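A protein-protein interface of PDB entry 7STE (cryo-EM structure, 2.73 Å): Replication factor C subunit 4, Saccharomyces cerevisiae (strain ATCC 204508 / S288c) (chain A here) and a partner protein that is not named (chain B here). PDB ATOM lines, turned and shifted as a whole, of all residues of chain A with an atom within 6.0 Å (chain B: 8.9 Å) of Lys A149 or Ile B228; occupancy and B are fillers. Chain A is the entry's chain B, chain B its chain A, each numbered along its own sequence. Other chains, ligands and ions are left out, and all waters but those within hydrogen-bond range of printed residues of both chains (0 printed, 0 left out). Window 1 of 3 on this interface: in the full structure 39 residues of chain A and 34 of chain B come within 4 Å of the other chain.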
ATOM      1  N   ASP A 117      21.702  21.616  12.488  1.00  0.00           N
ATOM      2  CA  ASP A 117      20.502  20.864  12.833  1.00  0.00           C
ATOM      3  C   ASP A 117      20.770  19.388  13.092  1.00  0.00           C
ATOM      4  O   ASP A 117      19.890  18.699  13.623  1.00  0.00           O
ATOM      5  CB  ASP A 117      19.465  20.990  11.714  1.00  0.00           C
ATOM      6  CG  ASP A 117      18.066  20.630  12.173  1.00  0.00           C
ATOM      7  OD1 ASP A 117      17.886  20.340  13.375  1.00  0.00           O
ATOM      8  OD2 ASP A 117      17.145  20.637  11.331  1.00  0.00           O
ATOM      9  N   SER A 118      21.951  18.887  12.738  1.00  0.00           N
ATOM     10  CA  SER A 118      22.313  17.484  12.922  1.00  0.00           C
ATOM     11  C   SER A 118      23.177  17.294  14.159  1.00  0.00           C
ATOM     12  O   SER A 118      24.102  16.476  14.167  1.00  0.00           O
ATOM     13  CB  SER A 118      23.029  16.957  11.682  1.00  0.00           C
ATOM     14  OG  SER A 118      24.344  17.479  11.594  1.00  0.00           O
ATOM     15  N   MET A 119      22.899  18.052  15.216  1.00  0.00           N
ATOM     16  CA  MET A 119      23.796  18.097  16.361  1.00  0.00           C
ATOM     17  C   MET A 119      22.989  18.419  17.616  1.00  0.00           C
ATOM     18  O   MET A 119      21.902  18.997  17.538  1.00  0.00           O
ATOM     19  CB  MET A 119      24.913  19.112  16.096  1.00  0.00           C
ATOM     20  CG  MET A 119      25.957  19.228  17.171  1.00  0.00           C
ATOM     21  SD  MET A 119      25.401  20.301  18.505  1.00  0.00           S
ATOM     22  CE  MET A 119      25.494  21.914  17.723  1.00  0.00           C
ATOM     23  N   THR A 120      23.537  18.036  18.770  1.00  0.00           N
ATOM     24  CA  THR A 120      22.774  17.955  20.009  1.00  0.00           C
ATOM     25  C   THR A 120      22.599  19.332  20.652  1.00  0.00           C
ATOM     26  O   THR A 120      23.222  20.321  20.263  1.00  0.00           O
ATOM     27  CB  THR A 120      23.452  17.006  20.998  1.00  0.00           C
ATOM     28  OG1 THR A 120      24.673  17.588  21.468  1.00  0.00           O
ATOM     29  CG2 THR A 120      23.749  15.657  20.346  1.00  0.00           C
ATOM     30  N   ALA A 121      21.734  19.380  21.670  1.00  0.00           N
ATOM     31  CA  ALA A 121      21.389  20.653  22.300  1.00  0.00           C
ATOM     32  C   ALA A 121      22.512  21.161  23.199  1.00  0.00           C
ATOM     33  O   ALA A 121      22.727  22.375  23.304  1.00  0.00           O
ATOM     34  CB  ALA A 121      20.097  20.505  23.100  1.00  0.00           C
ATOM     35  N   GLN A 124      24.837  22.996  21.244  1.00  0.00           N
ATOM     36  CA  GLN A 124      24.218  24.270  20.889  1.00  0.00           C
ATOM     37  C   GLN A 124      24.417  25.294  22.000  1.00  0.00           C
ATOM     38  O   GLN A 124      24.721  26.462  21.733  1.00  0.00           O
ATOM     39  CB  GLN A 124      22.728  24.090  20.600  1.00  0.00           C
ATOM     40  CG  GLN A 124      22.410  23.270  19.362  1.00  0.00           C
ATOM     41  CD  GLN A 124      21.004  23.517  18.844  1.00  0.00           C
ATOM     42  OE1 GLN A 124      20.370  24.516  19.183  1.00  0.00           O
ATOM     43  NE2 GLN A 124      20.508  22.601  18.021  1.00  0.00           N
ATOM     44  N   GLN A 146      15.772  23.251  10.024  1.00  0.00           N
ATOM     45  CA  GLN A 146      14.555  23.479  10.792  1.00  0.00           C
ATOM     46  C   GLN A 146      14.828  24.536  11.850  1.00  0.00           C
ATOM     47  O   GLN A 146      15.803  24.431  12.600  1.00  0.00           O
ATOM     48  CB  GLN A 146      14.067  22.183  11.451  1.00  0.00           C
ATOM     49  CG  GLN A 146      13.624  21.114  10.465  1.00  0.00           C
ATOM     50  CD  GLN A 146      12.404  21.528   9.665  1.00  0.00           C
ATOM     51  OE1 GLN A 146      12.492  21.782   8.464  1.00  0.00           O
ATOM     52  NE2 GLN A 146      11.256  21.596  10.330  1.00  0.00           N
ATOM     53  N   SER A 147      13.964  25.553  11.907  1.00  0.00           N
ATOM     54  CA  SER A 147      14.151  26.624  12.881  1.00  0.00           C
ATOM     55  C   SER A 147      13.781  26.167  14.287  1.00  0.00           C
ATOM     56  O   SER A 147      14.452  26.529  15.260  1.00  0.00           O
ATOM     57  CB  SER A 147      13.322  27.843  12.480  1.00  0.00           C
ATOM     58  OG  SER A 147      11.948  27.641  12.761  1.00  0.00           O
ATOM     59  N   ASN A 148      12.716  25.372  14.416  1.00  0.00           N
ATOM     60  CA  ASN A 148      12.269  24.945  15.737  1.00  0.00           C
ATOM     61  C   ASN A 148      13.270  24.004  16.396  1.00  0.00           C
ATOM     62  O   ASN A 148      13.331  23.936  17.630  1.00  0.00           O
ATOM     63  CB  ASN A 148      10.900  24.273  15.637  1.00  0.00           C
ATOM     64  CG  ASN A 148      10.906  23.066  14.719  1.00  0.00           C
ATOM     65  OD1 ASN A 148      11.947  22.678  14.189  1.00  0.00           O
ATOM     66  ND2 ASN A 148       9.737  22.465  14.527  1.00  0.00           N
ATOM     67  N   LYS A 149      14.056  23.274  15.603  1.00  0.00           N
ATOM     68  CA  LYS A 149      15.028  22.352  16.179  1.00  0.00           C
ATOM     69  C   LYS A 149      16.071  23.097  17.004  1.00  0.00           C
ATOM     70  O   LYS A 149      16.491  22.620  18.064  1.00  0.00           O
ATOM     71  CB  LYS A 149      15.698  21.536  15.074  1.00  0.00           C
ATOM     72  CG  LYS A 149      14.772  20.534  14.395  1.00  0.00           C
ATOM     73  CD  LYS A 149      14.475  19.328  15.283  1.00  0.00           C
ATOM     74  CE  LYS A 149      15.716  18.484  15.561  1.00  0.00           C
ATOM     75  NZ  LYS A 149      16.591  18.319  14.367  1.00  0.00           N
ATOM     76  N   ILE A 150      16.504  24.267  16.531  1.00  0.00           N
ATOM     77  CA  ILE A 150      17.464  25.060  17.286  1.00  0.00           C
ATOM     78  C   ILE A 150      16.852  25.462  18.619  1.00  0.00           C
ATOM     79  O   ILE A 150      15.667  25.813  18.704  1.00  0.00           O
ATOM     80  CB  ILE A 150      17.902  26.292  16.476  1.00  0.00           C
ATOM     81  CG1 ILE A 150      18.479  25.874  15.119  1.00  0.00           C
ATOM     82  CG2 ILE A 150      18.914  27.110  17.260  1.00  0.00           C
ATOM     83  CD1 ILE A 150      19.697  24.970  15.209  1.00  0.00           C
ATOM     84  N   ILE A 151      17.665  25.409  19.678  1.00  0.00           N
ATOM     85  CA  ILE A 151      17.158  25.688  21.014  1.00  0.00           C
ATOM     86  C   ILE A 151      16.587  27.103  21.078  1.00  0.00           C
ATOM     87  O   ILE A 151      16.979  27.996  20.317  1.00  0.00           O
ATOM     88  CB  ILE A 151      18.260  25.489  22.069  1.00  0.00           C
ATOM     89  CG1 ILE A 151      19.446  26.418  21.796  1.00  0.00           C
ATOM     90  CG2 ILE A 151      18.715  24.037  22.090  1.00  0.00           C
ATOM     91  CD1 ILE A 151      20.507  26.389  22.876  1.00  0.00           C
ATOM     92  N   GLU B 225      18.838  26.023  30.896  1.00  0.00           N
ATOM     93  CA  GLU B 225      18.018  24.894  30.478  1.00  0.00           C
ATOM     94  C   GLU B 225      17.570  25.076  29.034  1.00  0.00           C
ATOM     95  O   GLU B 225      17.027  26.125  28.671  1.00  0.00           O
ATOM     96  CB  GLU B 225      16.804  24.745  31.394  1.00  0.00           C
ATOM     97  CG  GLU B 225      17.156  24.396  32.832  1.00  0.00           C
ATOM     98  CD  GLU B 225      15.990  23.792  33.591  1.00  0.00           C
ATOM     99  OE1 GLU B 225      14.876  23.734  33.030  1.00  0.00           O
ATOM    100  OE2 GLU B 225      16.189  23.373  34.751  1.00  0.00           O
ATOM    101  N   CYS B 226      17.799  24.051  28.217  1.00  0.00           N
ATOM    102  CA  CYS B 226      17.377  24.056  26.826  1.00  0.00           C
ATOM    103  C   CYS B 226      17.153  22.620  26.380  1.00  0.00           C
ATOM    104  O   CYS B 226      17.790  21.693  26.887  1.00  0.00           O
ATOM    105  CB  CYS B 226      18.411  24.741  25.922  1.00  0.00           C
ATOM    106  SG  CYS B 226      20.109  24.177  26.180  1.00  0.00           S
ATOM    107  N   GLU B 227      16.241  22.444  25.427  1.00  0.00           N
ATOM    108  CA  GLU B 227      15.901  21.118  24.936  1.00  0.00           C
ATOM    109  C   GLU B 227      15.446  21.218  23.488  1.00  0.00           C
ATOM    110  O   GLU B 227      15.032  22.280  23.017  1.00  0.00           O
ATOM    111  CB  GLU B 227      14.814  20.463  25.797  1.00  0.00           C
ATOM    112  CG  GLU B 227      13.498  21.224  25.823  1.00  0.00           C
ATOM    113  CD  GLU B 227      12.537  20.691  26.867  1.00  0.00           C
ATOM    114  OE1 GLU B 227      12.917  19.761  27.608  1.00  0.00           O
ATOM    115  OE2 GLU B 227      11.400  21.203  26.948  1.00  0.00           O
ATOM    116  N   ILE B 228      15.526  20.090  22.788  1.00  0.00           N
ATOM    117  CA  ILE B 228      15.121  20.003  21.388  1.00  0.00           C
ATOM    118  C   ILE B 228      14.175  18.817  21.233  1.00  0.00           C
ATOM    119  O   ILE B 228      14.604  17.737  20.802  1.00  0.00           O
ATOM    120  CB  ILE B 228      16.337  19.867  20.457  1.00  0.00           C
ATOM    121  CG1 ILE B 228      17.302  21.039  20.663  1.00  0.00           C
ATOM    122  CG2 ILE B 228      15.886  19.800  19.002  1.00  0.00           C
ATOM    123  CD1 ILE B 228      18.644  20.854  19.983  1.00  0.00           C
ATOM    124  N   PRO B 229      12.884  18.961  21.573  1.00  0.00           N
ATOM    125  CA  PRO B 229      11.931  17.855  21.462  1.00  0.00           C
ATOM    126  C   PRO B 229      11.384  17.687  20.047  1.00  0.00           C
ATOM    127  O   PRO B 229      11.440  18.639  19.269  1.00  0.00           O
ATOM    128  CB  PRO B 229      10.820  18.254  22.433  1.00  0.00           C
ATOM    129  CG  PRO B 229      10.869  19.749  22.488  1.00  0.00           C
ATOM    130  CD  PRO B 229      12.245  20.197  22.058  1.00  0.00           C
ATOM    131  N   GLY B 239      17.487  11.812  28.045  1.00  0.00           N
ATOM    132  CA  GLY B 239      18.889  11.793  27.673  1.00  0.00           C
ATOM    133  C   GLY B 239      19.502  13.179  27.628  1.00  0.00           C
ATOM    134  O   GLY B 239      18.791  14.180  27.538  1.00  0.00           O
ATOM    135  N   ILE B 240      20.834  13.235  27.692  1.00  0.00           N
ATOM    136  CA  ILE B 240      21.521  14.522  27.656  1.00  0.00           C
ATOM    137  C   ILE B 240      21.314  15.201  26.308  1.00  0.00           C
ATOM    138  O   ILE B 240      21.196  16.429  26.227  1.00  0.00           O
ATOM    139  CB  ILE B 240      23.017  14.337  27.973  1.00  0.00           C
ATOM    140  CG1 ILE B 240      23.699  15.697  28.132  1.00  0.00           C
ATOM    141  CG2 ILE B 240      23.704  13.525  26.882  1.00  0.00           C
ATOM    142  CD1 ILE B 240      24.992  15.639  28.915  1.00  0.00           C
ATOM    143  N   ASP B 241      21.270  14.417  25.228  1.00  0.00           N
ATOM    144  CA  ASP B 241      21.063  15.000  23.906  1.00  0.00           C
ATOM    145  C   ASP B 241      19.706  15.685  23.811  1.00  0.00           C
ATOM    146  O   ASP B 241      19.597  16.791  23.268  1.00  0.00           O
ATOM    147  CB  ASP B 241      21.193  13.919  22.831  1.00  0.00           C
ATOM    148  CG  ASP B 241      20.289  12.729  23.087  1.00  0.00           C
ATOM    149  OD1 ASP B 241      20.323  12.185  24.212  1.00  0.00           O
ATOM    150  OD2 ASP B 241      19.543  12.338  22.165  1.00  0.00           O
ATOM    151  N   TYR B 242      18.658  15.045  24.334  1.00  0.00           N
ATOM    152  CA  TYR B 242      17.324  15.634  24.270  1.00  0.00           C
ATOM    153  C   TYR B 242      17.252  16.918  25.086  1.00  0.00           C
ATOM    154  O   TYR B 242      16.705  17.929  24.629  1.00  0.00           O
ATOM    155  CB  TYR B 242      16.283  14.627  24.765  1.00  0.00           C
ATOM    156  CG  TYR B 242      15.939  13.535  23.774  1.00  0.00           C
ATOM    157  CD1 TYR B 242      15.724  13.823  22.431  1.00  0.00           C
ATOM    158  CD2 TYR B 242      15.825  12.213  24.183  1.00  0.00           C
ATOM    159  CE1 TYR B 242      15.408  12.827  21.527  1.00  0.00           C
ATOM    160  CE2 TYR B 242      15.509  11.210  23.286  1.00  0.00           C
ATOM    161  CZ  TYR B 242      15.302  11.523  21.959  1.00  0.00           C
ATOM    162  OH  TYR B 242      14.989  10.528  21.063  1.00  0.00           O
ATOM    163  N   THR B 243      17.800  16.898  26.300  1.00  0.00           N
ATOM    164  CA  THR B 243      17.739  18.043  27.196  1.00  0.00           C
ATOM    165  C   THR B 243      19.053  18.165  27.952  1.00  0.00           C
ATOM    166  O   THR B 243      19.721  17.167  28.234  1.00  0.00           O
ATOM    167  CB  THR B 243      16.577  17.917  28.193  1.00  0.00           C
ATOM    168  OG1 THR B 243      15.373  17.581  27.491  1.00  0.00           O
ATOM    169  CG2 THR B 243      16.372  19.221  28.950  1.00  0.00           C
ATOM    170  N   PHE B 244      19.415  19.405  28.282  1.00  0.00           N
ATOM    171  CA  PHE B 244      20.618  19.674  29.060  1.00  0.00           C
ATOM    172  C   PHE B 244      20.250  20.429  30.331  1.00  0.00           C
ATOM    173  O   PHE B 244      20.921  21.396  30.706  1.00  0.00           O
ATOM    174  CB  PHE B 244      21.632  20.468  28.234  1.00  0.00           C
ATOM    175  CG  PHE B 244      23.016  20.483  28.822  1.00  0.00           C
ATOM    176  CD1 PHE B 244      23.830  19.365  28.739  1.00  0.00           C
ATOM    177  CD2 PHE B 244      23.504  21.613  29.457  1.00  0.00           C
ATOM    178  CE1 PHE B 244      25.103  19.375  29.279  1.00  0.00           C
ATOM    179  CE2 PHE B 244      24.775  21.629  29.998  1.00  0.00           C
ATOM    180  CZ  PHE B 244      25.574  20.509  29.909  1.00  0.00           C
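The side-chain amino group (NZ) of Lys A149 lies within salt-bridge range of the side-chain carboxylate (OD1) of Asp A117 (2.6 Å). OE1 of Gln A124 lies within hydrogen-bond range of N of Ile A151 (2.9 Å). The backbone carbonyl oxygen of Cys B226 is in hydrogen-bond range of the backbone NH of Phe B244 (3.1 Å). N of Ile B228 sits at hydrogen-bond distance from O of Tyr B242.
Among the printed residues, merely in contact across the chains: Thr A120 with Asp B241, Ala A121 with Ile B228, Ala A121 with Asp B241, Gln A124 with Ile B228, Lys A149 with Ile B228, Ile A151 with Cys B226 and Ile A151 with Ile B228.
Asp A117 touches none of the printed residues of chain B. Of the printed residues of chain B, Thr A120 touches Asp B241. Printed residues of chain B within 4 Å of Ala A121: Ile B228 and Asp B241. No residue of chain B comes within 4 Å of Asn A148. Of the printed residues of chain B, Lys A149 touches Ile B228. Of the printed residues of chain B, Ile A151 touches Cys B226 and Ile B228. Glu B225 touches none of the printed residues of chain A. Of the printed residues of chain A, Cys B226 touches Ile A151 (3.9 Å). Ile B228 touches just these residues of chain A: Ala A121, Gln A124, Lys A149 and Ile A151. The nearest printed residue of chain B that does not touch Ile A151 is Glu B227 (4.2 Å).
Of the 12 printed residues of chain A, 5 touch a printed residue of chain B. Printed residues of chain A that touch a printed residue of chain B: Thr A120, Ala A121, Gln A124, Lys A149 and Ile A151. Hydrophobic or aromatic side chains of chain B that line the printed part of chain A: Ile B228. Along chain B the printed residues that touch a printed residue of chain A span positions 226 to 241. Among the printed residues, no Asp or Glu carboxylate lies within 4 Å of a Lys or Arg side-chain nitrogen of the other chain.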
